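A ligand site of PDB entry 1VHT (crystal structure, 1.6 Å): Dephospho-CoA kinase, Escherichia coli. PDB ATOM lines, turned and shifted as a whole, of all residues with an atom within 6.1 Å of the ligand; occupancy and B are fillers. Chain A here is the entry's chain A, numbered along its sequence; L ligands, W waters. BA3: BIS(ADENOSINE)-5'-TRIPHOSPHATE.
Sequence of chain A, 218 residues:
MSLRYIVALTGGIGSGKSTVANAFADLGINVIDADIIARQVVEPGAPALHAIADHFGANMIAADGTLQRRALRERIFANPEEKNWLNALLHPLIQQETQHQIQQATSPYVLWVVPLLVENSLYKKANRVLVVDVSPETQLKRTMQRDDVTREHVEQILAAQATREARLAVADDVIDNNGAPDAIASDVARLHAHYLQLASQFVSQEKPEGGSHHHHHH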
ATOM      1  N   GLY A  11       9.861  30.507   6.646  1.00  0.00           N
ATOM      2  CA  GLY A  11      10.597  29.237   6.578  1.00  0.00           C
ATOM      3  C   GLY A  11      10.059  28.374   7.728  1.00  0.00           C
ATOM      4  O   GLY A  11       9.464  28.896   8.671  1.00  0.00           O
ATOM      5  N   GLY A  12      10.269  27.067   7.593  1.00  0.00           N
ATOM      6  CA  GLY A  12       9.711  26.212   8.680  1.00  0.00           C
ATOM      7  C   GLY A  12      10.648  26.161   9.868  1.00  0.00           C
ATOM      8  O   GLY A  12      11.695  26.795   9.926  1.00  0.00           O
ATOM      9  N   ILE A  13      10.213  25.403  10.901  1.00  0.00           N
ATOM     10  CA  ILE A  13      11.057  25.269  12.091  1.00  0.00           C
ATOM     11  C   ILE A  13      12.434  24.734  11.720  1.00  0.00           C
ATOM     12  O   ILE A  13      12.638  23.833  10.915  1.00  0.00           O
ATOM     13  CB  ILE A  13      10.404  24.345  13.147  1.00  0.00           C
ATOM     14  CG1 ILE A  13      11.102  24.452  14.494  1.00  0.00           C
ATOM     15  CG2 ILE A  13      10.285  22.917  12.663  1.00  0.00           C
ATOM     16  CD1 ILE A  13      10.248  23.761  15.580  1.00  0.00           C
ATOM     17  N   GLY A  14      13.432  25.414  12.317  1.00  0.00           N
ATOM     18  CA  GLY A  14      14.820  25.098  12.177  1.00  0.00           C
ATOM     19  C   GLY A  14      15.431  25.503  10.854  1.00  0.00           C
ATOM     20  O   GLY A  14      16.567  25.132  10.598  1.00  0.00           O
ATOM     21  N   SER A  15      14.761  26.354  10.083  1.00  0.00           N
ATOM     22  CA  SER A  15      15.313  26.714   8.772  1.00  0.00           C
ATOM     23  C   SER A  15      16.328  27.852   8.849  1.00  0.00           C
ATOM     24  O   SER A  15      17.180  27.903   7.947  1.00  0.00           O
ATOM     25  CB  SER A  15      14.179  27.045   7.777  1.00  0.00           C
ATOM     26  OG  SER A  15      13.373  28.091   8.277  1.00  0.00           O
ATOM     27  N   GLY A  16      16.222  28.709   9.840  1.00  0.00           N
ATOM     28  CA  GLY A  16      17.173  29.809   9.983  1.00  0.00           C
ATOM     29  C   GLY A  16      16.594  31.181   9.703  1.00  0.00           C
ATOM     30  O   GLY A  16      17.321  32.052   9.189  1.00  0.00           O
ATOM     31  N   LYS A  17      15.304  31.343   9.940  1.00  0.00           N
ATOM     32  CA  LYS A  17      14.655  32.639   9.741  1.00  0.00           C
ATOM     33  C   LYS A  17      15.405  33.760  10.447  1.00  0.00           C
ATOM     34  O   LYS A  17      15.734  34.751   9.801  1.00  0.00           O
ATOM     35  CB  LYS A  17      13.223  32.643  10.294  1.00  0.00           C
ATOM     36  CG  LYS A  17      12.270  31.824   9.425  1.00  0.00           C
ATOM     37  CD  LYS A  17      10.878  31.817  10.017  1.00  0.00           C
ATOM     38  CE  LYS A  17      10.858  30.989  11.285  1.00  0.00           C
ATOM     39  NZ  LYS A  17      11.146  29.556  11.096  1.00  0.00           N
ATOM     40  N   SER A  18      15.731  33.608  11.733  1.00  0.00           N
ATOM     41  CA  SER A  18      16.410  34.704  12.446  1.00  0.00           C
ATOM     42  C   SER A  18      17.843  34.884  11.970  1.00  0.00           C
ATOM     43  O   SER A  18      18.354  36.012  11.906  1.00  0.00           O
ATOM     44  CB  SER A  18      16.358  34.383  13.956  1.00  0.00           C
ATOM     45  OG  SER A  18      14.980  34.530  14.328  1.00  0.00           O
ATOM     46  N   THR A  19      18.497  33.793  11.616  1.00  0.00           N
ATOM     47  CA  THR A  19      19.857  33.836  11.067  1.00  0.00           C
ATOM     48  C   THR A  19      19.895  34.698   9.811  1.00  0.00           C
ATOM     49  O   THR A  19      20.738  35.591   9.700  1.00  0.00           O
ATOM     50  CB  THR A  19      20.331  32.399  10.788  1.00  0.00           C
ATOM     51  OG1 THR A  19      20.349  31.735  12.070  1.00  0.00           O
ATOM     52  CG2 THR A  19      21.758  32.379  10.253  1.00  0.00           C
ATOM     53  N   VAL A  20      19.007  34.385   8.851  1.00  0.00           N
ATOM     54  CA  VAL A  20      18.958  35.232   7.630  1.00  0.00           C
ATOM     55  C   VAL A  20      18.524  36.644   7.958  1.00  0.00           C
ATOM     56  O   VAL A  20      19.050  37.630   7.440  1.00  0.00           O
ATOM     57  CB  VAL A  20      17.967  34.555   6.647  1.00  0.00           C
ATOM     58  CG1 VAL A  20      17.731  35.441   5.419  1.00  0.00           C
ATOM     59  CG2 VAL A  20      18.487  33.187   6.208  1.00  0.00           C
ATOM     60  N   PRO A 115       6.708  33.627  10.778  1.00  0.00           N
ATOM     61  CA  PRO A 115       6.685  32.173  10.728  1.00  0.00           C
ATOM     62  C   PRO A 115       5.411  31.624  10.124  1.00  0.00           C
ATOM     63  O   PRO A 115       5.510  30.601   9.412  1.00  0.00           O
ATOM     64  CB  PRO A 115       6.768  31.813  12.219  1.00  0.00           C
ATOM     65  CG  PRO A 115       7.581  32.942  12.811  1.00  0.00           C
ATOM     66  CD  PRO A 115       7.030  34.184  12.096  1.00  0.00           C
ATOM     67  N   VAL A 132      13.403  31.013   3.415  1.00  0.00           N
ATOM     68  CA  VAL A 132      14.707  30.388   3.735  1.00  0.00           C
ATOM     69  C   VAL A 132      14.368  28.887   3.740  1.00  0.00           C
ATOM     70  O   VAL A 132      13.464  28.448   4.484  1.00  0.00           O
ATOM     71  CB  VAL A 132      15.367  30.886   4.997  1.00  0.00           C
ATOM     72  CG1 VAL A 132      14.442  30.872   6.201  1.00  0.00           C
ATOM     73  CG2 VAL A 132      16.663  30.112   5.284  1.00  0.00           C
ATOM     74  N   ARG A 142      18.667  20.210  13.291  1.00  0.00           N
ATOM     75  CA  ARG A 142      18.968  21.469  13.988  1.00  0.00           C
ATOM     76  C   ARG A 142      18.049  21.726  15.148  1.00  0.00           C
ATOM     77  O   ARG A 142      18.513  22.236  16.195  1.00  0.00           O
ATOM     78  CB  ARG A 142      18.951  22.627  12.972  1.00  0.00           C
ATOM     79  CG  ARG A 142      20.090  22.540  11.980  1.00  0.00           C
ATOM     80  CD  ARG A 142      20.211  23.758  11.060  1.00  0.00           C
ATOM     81  NE  ARG A 142      21.219  23.525  10.035  1.00  0.00           N
ATOM     82  CZ  ARG A 142      21.307  24.256   8.910  1.00  0.00           C
ATOM     83  NH1 ARG A 142      20.442  25.240   8.707  1.00  0.00           N
ATOM     84  NH2 ARG A 142      22.233  23.975   8.007  1.00  0.00           N
ATOM     85  N   THR A 143      16.773  21.411  15.049  1.00  0.00           N
ATOM     86  CA  THR A 143      15.833  21.640  16.151  1.00  0.00           C
ATOM     87  C   THR A 143      16.125  20.673  17.297  1.00  0.00           C
ATOM     88  O   THR A 143      16.058  21.031  18.474  1.00  0.00           O
ATOM     89  CB  THR A 143      14.388  21.553  15.686  1.00  0.00           C
ATOM     90  OG1 THR A 143      14.209  22.492  14.591  1.00  0.00           O
ATOM     91  CG2 THR A 143      13.445  21.928  16.814  1.00  0.00           C
ATOM     92  N   ARG A 146      19.266  22.036  19.060  1.00  0.00           N
ATOM     93  CA  ARG A 146      18.956  23.245  19.815  1.00  0.00           C
ATOM     94  C   ARG A 146      18.179  22.979  21.085  1.00  0.00           C
ATOM     95  O   ARG A 146      18.576  23.442  22.162  1.00  0.00           O
ATOM     96  CB  ARG A 146      18.186  24.229  18.911  1.00  0.00           C
ATOM     97  CG  ARG A 146      17.937  25.591  19.545  1.00  0.00           C
ATOM     98  CD  ARG A 146      16.858  26.335  18.767  1.00  0.00           C
ATOM     99  NE  ARG A 146      16.829  27.765  19.091  1.00  0.00           N
ATOM    100  CZ  ARG A 146      16.066  28.294  20.055  1.00  0.00           C
ATOM    101  NH1 ARG A 146      15.281  27.506  20.784  1.00  0.00           N
ATOM    102  NH2 ARG A 146      16.104  29.595  20.285  1.00  0.00           N
ATOM    103  N   ASP A 147      17.080  22.250  21.003  1.00  0.00           N
ATOM    104  CA  ASP A 147      16.232  21.992  22.151  1.00  0.00           C
ATOM    105  C   ASP A 147      16.487  20.687  22.873  1.00  0.00           C
ATOM    106  O   ASP A 147      15.813  20.415  23.880  1.00  0.00           O
ATOM    107  CB  ASP A 147      14.759  22.022  21.695  1.00  0.00           C
ATOM    108  CG  ASP A 147      14.380  23.339  21.049  1.00  0.00           C
ATOM    109  OD1 ASP A 147      15.073  24.351  21.314  1.00  0.00           O
ATOM    110  OD2 ASP A 147      13.399  23.370  20.282  1.00  0.00           O
ATOM    111  N   HIS A 153       9.450  14.427  18.281  1.00  0.00           N
ATOM    112  CA  HIS A 153       8.881  15.681  18.750  1.00  0.00           C
ATOM    113  C   HIS A 153       8.915  16.741  17.637  1.00  0.00           C
ATOM    114  O   HIS A 153       7.917  17.404  17.401  1.00  0.00           O
ATOM    115  CB  HIS A 153       9.612  16.190  19.980  1.00  0.00           C
ATOM    116  CG  HIS A 153       9.067  17.416  20.625  1.00  0.00           C
ATOM    117  ND1 HIS A 153       7.969  17.410  21.458  1.00  0.00           N
ATOM    118  CD2 HIS A 153       9.474  18.714  20.562  1.00  0.00           C
ATOM    119  CE1 HIS A 153       7.726  18.632  21.879  1.00  0.00           C
ATOM    120  NE2 HIS A 153       8.627  19.454  21.354  1.00  0.00           N
ATOM    121  N   ILE A 157       5.866  18.767  14.947  1.00  0.00           N
ATOM    122  CA  ILE A 157       5.800  20.178  14.583  1.00  0.00           C
ATOM    123  C   ILE A 157       5.850  20.316  13.062  1.00  0.00           C
ATOM    124  O   ILE A 157       5.075  21.091  12.489  1.00  0.00           O
ATOM    125  CB  ILE A 157       6.945  20.993  15.220  1.00  0.00           C
ATOM    126  CG1 ILE A 157       6.849  20.924  16.748  1.00  0.00           C
ATOM    127  CG2 ILE A 157       6.923  22.436  14.769  1.00  0.00           C
ATOM    128  CD1 ILE A 157       8.126  21.365  17.452  1.00  0.00           C
ATOM    129  N   GLN A 161       2.972  22.287  10.548  1.00  0.00           N
ATOM    130  CA  GLN A 161       3.294  23.479   9.777  1.00  0.00           C
ATOM    131  C   GLN A 161       3.011  23.245   8.290  1.00  0.00           C
ATOM    132  O   GLN A 161       2.852  22.100   7.864  1.00  0.00           O
ATOM    133  CB  GLN A 161       4.821  23.751   9.902  1.00  0.00           C
ATOM    134  CG  GLN A 161       5.160  24.153  11.334  1.00  0.00           C
ATOM    135  CD  GLN A 161       6.539  24.752  11.480  1.00  0.00           C
ATOM    136  OE1 GLN A 161       7.470  24.460  10.734  1.00  0.00           O
ATOM    137  NE2 GLN A 161       6.682  25.616  12.491  1.00  0.00           N
ATOM    138  N   ASN A 177      19.751  27.385   3.159  1.00  0.00           N
ATOM    139  CA  ASN A 177      20.504  27.498   4.411  1.00  0.00           C
ATOM    140  C   ASN A 177      20.916  26.085   4.851  1.00  0.00           C
ATOM    141  O   ASN A 177      20.977  25.788   6.028  1.00  0.00           O
ATOM    142  CB  ASN A 177      19.754  28.223   5.503  1.00  0.00           C
ATOM    143  CG  ASN A 177      20.572  28.558   6.733  1.00  0.00           C
ATOM    144  OD1 ASN A 177      21.791  28.798   6.663  1.00  0.00           O
ATOM    145  ND2 ASN A 177      19.953  28.529   7.904  1.00  0.00           N
ATOM    146  N   ASN A 178      21.067  25.218   3.858  1.00  0.00           N
ATOM    147  CA  ASN A 178      21.462  23.835   4.170  1.00  0.00           C
ATOM    148  C   ASN A 178      22.950  23.807   4.499  1.00  0.00           C
ATOM    149  O   ASN A 178      23.421  23.014   5.327  1.00  0.00           O
ATOM    150  CB  ASN A 178      21.152  22.903   3.028  1.00  0.00           C
ATOM    151  CG  ASN A 178      19.807  22.221   3.067  1.00  0.00           C
ATOM    152  OD1 ASN A 178      19.404  21.632   4.078  1.00  0.00           O
ATOM    153  ND2 ASN A 178      19.095  22.288   1.943  1.00  0.00           N
ATOM    154  N   GLY A 179      23.704  24.661   3.830  1.00  0.00           N
ATOM    155  CA  GLY A 179      25.145  24.750   4.027  1.00  0.00           C
ATOM    156  C   GLY A 179      25.503  25.201   5.429  1.00  0.00           C
ATOM    157  O   GLY A 179      24.708  25.158   6.358  1.00  0.00           O
ATOM    158  N   ALA A 180      26.739  25.674   5.570  1.00  0.00           N
ATOM    159  CA  ALA A 180      27.226  26.142   6.868  1.00  0.00           C
ATOM    160  C   ALA A 180      26.756  27.551   7.124  1.00  0.00           C
ATOM    161  O   ALA A 180      26.325  28.280   6.220  1.00  0.00           O
ATOM    162  CB  ALA A 180      28.740  26.022   6.921  1.00  0.00           C
ATOM    163  N   PRO A 181      26.977  28.072   8.323  1.00  0.00           N
ATOM    164  CA  PRO A 181      26.556  29.414   8.662  1.00  0.00           C
ATOM    165  C   PRO A 181      27.135  30.542   7.838  1.00  0.00           C
ATOM    166  O   PRO A 181      26.855  31.716   8.181  1.00  0.00           O
ATOM    167  CB  PRO A 181      26.914  29.544  10.139  1.00  0.00           C
ATOM    168  CG  PRO A 181      27.063  28.165  10.658  1.00  0.00           C
ATOM    169  CD  PRO A 181      27.496  27.311   9.489  1.00  0.00           C
ATOM    170  N   ASP A 182      27.835  30.337   6.713  1.00  0.00           N
ATOM    171  CA  ASP A 182      28.425  31.373   5.930  1.00  0.00           C
ATOM    172  C   ASP A 182      28.192  31.518   4.465  1.00  0.00           C
ATOM    173  O   ASP A 182      28.848  32.450   3.913  1.00  0.00           O
ATOM    174  CB  ASP A 182      29.967  31.322   6.182  1.00  0.00           C
ATOM    175  N   ILE A 184      25.436  32.284   3.445  1.00  0.00           N
ATOM    176  CA  ILE A 184      24.331  33.174   3.652  1.00  0.00           C
ATOM    177  C   ILE A 184      24.728  34.597   3.287  1.00  0.00           C
ATOM    178  O   ILE A 184      23.958  35.225   2.588  1.00  0.00           O
ATOM    179  CB  ILE A 184      23.882  33.135   5.137  1.00  0.00           C
ATOM    180  CG1 ILE A 184      23.276  31.759   5.407  1.00  0.00           C
ATOM    181  CG2 ILE A 184      22.950  34.241   5.516  1.00  0.00           C
ATOM    182  CD1 ILE A 184      22.071  31.430   4.583  1.00  0.00           C
HETATM  183  N9A BA3 L   1      21.448  27.248  12.519  1.00  0.00           N
HETATM  184  C8A BA3 L   1      21.051  28.279  11.675  1.00  0.00           C
HETATM  185  N7A BA3 L   1      21.687  28.335  10.537  1.00  0.00           N
HETATM  186  C5A BA3 L   1      22.542  27.260  10.581  1.00  0.00           C
HETATM  187  C6A BA3 L   1      23.440  26.831   9.637  1.00  0.00           C
HETATM  188  N6A BA3 L   1      23.609  27.350   8.561  1.00  0.00           N
HETATM  189  N1A BA3 L   1      24.181  25.701   9.999  1.00  0.00           N
HETATM  190  C2A BA3 L   1      24.002  25.086  11.192  1.00  0.00           C
HETATM  191  N3A BA3 L   1      23.141  25.479  12.117  1.00  0.00           N
HETATM  192  C4A BA3 L   1      22.427  26.573  11.753  1.00  0.00           C
HETATM  193  O5B BA3 L   1      18.034  28.846  13.717  1.00  0.00           O
HETATM  194  C5B BA3 L   1      17.611  27.677  14.432  1.00  0.00           C
HETATM  195  C4B BA3 L   1      18.735  26.830  14.774  1.00  0.00           C
HETATM  196  O4B BA3 L   1      19.519  26.465  13.682  1.00  0.00           O
HETATM  197  C3B BA3 L   1      19.592  27.537  15.763  1.00  0.00           C
HETATM  198  O3B BA3 L   1      20.075  26.574  16.722  1.00  0.00           O
HETATM  199  C2B BA3 L   1      20.639  28.072  14.975  1.00  0.00           C
HETATM  200  O2B BA3 L   1      21.845  28.246  15.704  1.00  0.00           O
HETATM  201  C1B BA3 L   1      20.848  26.934  13.868  1.00  0.00           C
HETATM  202  PE  BA3 L   1      17.138  30.132  13.800  1.00  0.00           P
HETATM  203  O1E BA3 L   1      16.743  30.436  15.171  1.00  0.00           O
HETATM  204  O2E BA3 L   1      17.803  31.158  12.940  1.00  0.00           O
HETATM  205  O3E BA3 L   1      15.908  29.593  13.007  1.00  0.00           O
HETATM  206  PF  BA3 L   1      14.460  30.073  12.904  1.00  0.00           P
HETATM  207  O1F BA3 L   1      13.984  29.484  11.664  1.00  0.00           O
HETATM  208  O2F BA3 L   1      14.431  31.546  13.110  1.00  0.00           O
HETATM  209  O3F BA3 L   1      13.721  29.473  14.166  1.00  0.00           O
HETATM  210  PG  BA3 L   1      12.691  28.358  14.474  1.00  0.00           P
HETATM  211  O1G BA3 L   1      13.491  27.017  14.384  1.00  0.00           O
HETATM  212  O2G BA3 L   1      11.444  28.362  13.667  1.00  0.00           O
HETATM  213  O5D BA3 L   1      12.364  28.499  16.038  1.00  0.00           O
HETATM  214  C5D BA3 L   1      13.483  28.405  17.018  1.00  0.00           C
HETATM  215  C4D BA3 L   1      12.924  27.641  18.348  1.00  0.00           C
HETATM  216  O4D BA3 L   1      11.575  28.087  18.600  1.00  0.00           O
HETATM  217  C3D BA3 L   1      12.727  26.158  18.000  1.00  0.00           C
HETATM  218  O3D BA3 L   1      13.948  25.429  18.168  1.00  0.00           O
HETATM  219  C2D BA3 L   1      11.746  25.754  19.023  1.00  0.00           C
HETATM  220  O2D BA3 L   1      12.473  25.817  20.257  1.00  0.00           O
HETATM  221  C1D BA3 L   1      10.757  26.977  18.954  1.00  0.00           C
HETATM  222  N9G BA3 L   1       9.564  26.848  18.047  1.00  0.00           N
HETATM  223  C8G BA3 L   1       9.300  27.574  16.911  1.00  0.00           C
HETATM  224  N7G BA3 L   1       8.200  27.320  16.290  1.00  0.00           N
HETATM  225  C5G BA3 L   1       7.635  26.327  17.079  1.00  0.00           C
HETATM  226  C6G BA3 L   1       6.387  25.631  16.918  1.00  0.00           C
HETATM  227  N6G BA3 L   1       5.585  25.801  15.997  1.00  0.00           N
HETATM  228  N1G BA3 L   1       6.180  24.691  17.940  1.00  0.00           N
HETATM  229  C2G BA3 L   1       7.042  24.451  19.004  1.00  0.00           C
HETATM  230  N3G BA3 L   1       8.220  25.121  19.140  1.00  0.00           N
HETATM  231  C4G BA3 L   1       8.442  26.035  18.167  1.00  0.00           C
HETATM  232  O   HOH W   1      18.846  26.594  10.568  1.00  0.00           O
HETATM  233  O   HOH W   2      13.158  32.837  14.817  1.00  0.00           O
HETATM  234  O   HOH W   3      14.728  31.891  16.486  1.00  0.00           O
HETATM  235  O   HOH W   4      15.362  25.113  15.600  1.00  0.00           O
HETATM  236  O   HOH W   5      22.970  23.680  14.185  1.00  0.00           O
HETATM  237  O   HOH W   6      20.883  23.941  16.146  1.00  0.00           O
HETATM  238  O   HOH W   7       8.891  27.245  13.683  1.00  0.00           O
HETATM  239  O   HOH W   8       9.771  30.738  14.748  1.00  0.00           O
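An oxygen (O1F) of the ligand lies within hydrogen-bond range of the backbone NH of Gly 16 (3.0 Å).
OD1 of Asn 177 is in hydrogen-bond range of N6A of the ligand, at 3.0 Å.
The backbone NH of Lys 17 lies within hydrogen-bond range of an oxygen (O1F) of the ligand, 2.9 Å away.
An oxygen (O2E) of the ligand lies within hydrogen-bond range of the backbone NH of Thr 19 (3.0 Å).
An oxygen (O2F) of the ligand sits at hydrogen-bond distance from the side-chain hydroxyl of Ser 18 (3.3 Å).
The side-chain hydroxyl of Thr 19 sits at hydrogen-bond distance from an oxygen (O2E) of the ligand, 2.8 Å away.
NH1 of Arg 146 lies within hydrogen-bond range of O2D of the ligand, 3.3 Å away.
An oxygen (O2F) of the ligand lies within hydrogen-bond range of the backbone NH of Ser 18 (2.8 Å).
N of Gly 14 sits at hydrogen-bond distance from O1G of the ligand.
A nitrogen (N6A) of the ligand is in hydrogen-bond range of the backbone carbonyl oxygen (O) of Gly 179 (3.3 Å).
An oxygen (O2G) of the ligand lies within salt-bridge range of the side-chain amino group (NZ) of Lys 17 (2.9 Å).
A nitrogen (N1A) of the ligand sits at hydrogen-bond distance from the guanidinium group (NH2) of Arg 142, at 3.3 Å.
OD2 of Asp 147 is in hydrogen-bond range of O2D of the ligand (2.6 Å).
The backbone carbonyl oxygen (O) of Gly 179 is in hydrogen-bond range of the guanidinium group (NH2) of Arg 142 (3.2 Å).
The side-chain amide nitrogen (ND2) of Asn 177 sits at hydrogen-bond distance from the backbone carbonyl oxygen (O) of Ser 15 (2.8 Å).
O of Gly 12 is in hydrogen-bond range of OG of Ser 15.
The guanidinium group (NH1) of Arg 146 is in salt-bridge range of the side-chain carboxylate (OD1) of Asp 147, at 3.2 Å.
The side-chain amide oxygen of Gln 161 is in hydrogen-bond range of the backbone NH of Ile 13 (2.9 Å).
The backbone carbonyl oxygen (O) of Asn 178 sits at hydrogen-bond distance from the guanidinium group (NH2) of Arg 142 (3.1 Å).
The guanidinium group (NH1) of Arg 142 is in hydrogen-bond range of the backbone carbonyl oxygen (O) of Asn 177 (2.8 Å).
The side-chain amino group of Lys 17 is in hydrogen-bond range of the backbone carbonyl oxygen of Gly 12 (3.0 Å).
N of Pro 181 sits close to N6A of the ligand (3.5 Å).
Gly 12 touches the ligand.
Ile 13 touches the ligand.
Ser 15 touches the ligand.
CG2 of Thr 143 touches O3D of the ligand, at 3.8 Å.
Ile 157 touches the ligand (CD1 to C2G, 3.6 Å).
Gln 161 touches the ligand (NE2 to N6G, 3.7 Å).
C of Ala 180 touches N6A of the ligand (3.5 Å).
Hydrophobic or aromatic side chains that line the ligand: Ile 13, Ile 157 and Pro 181.
The nearest printed residue that does not touch the ligand is Val 20 (5.3 Å).
Water W2 bridges an oxygen (O2F) of the ligand (2.5 Å) and the side-chain hydroxyl of Ser 18 (2.5 Å).
Water W7 lies within hydrogen-bond range of N7G of the ligand (2.7 Å) and NE2 of Gln 161 (3.0 Å).
Water W3 lies within hydrogen-bond range of O1E of the ligand and OG of Ser 18.
Water W6 lies within hydrogen-bond range of an oxygen (O3B) of the ligand (2.8 Å) and the backbone carbonyl oxygen of Arg 142 (2.9 Å).
Water W4 lies within hydrogen-bond range of O1G of the ligand (2.9 Å) and OG1 of Thr 143 (3.0 Å).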
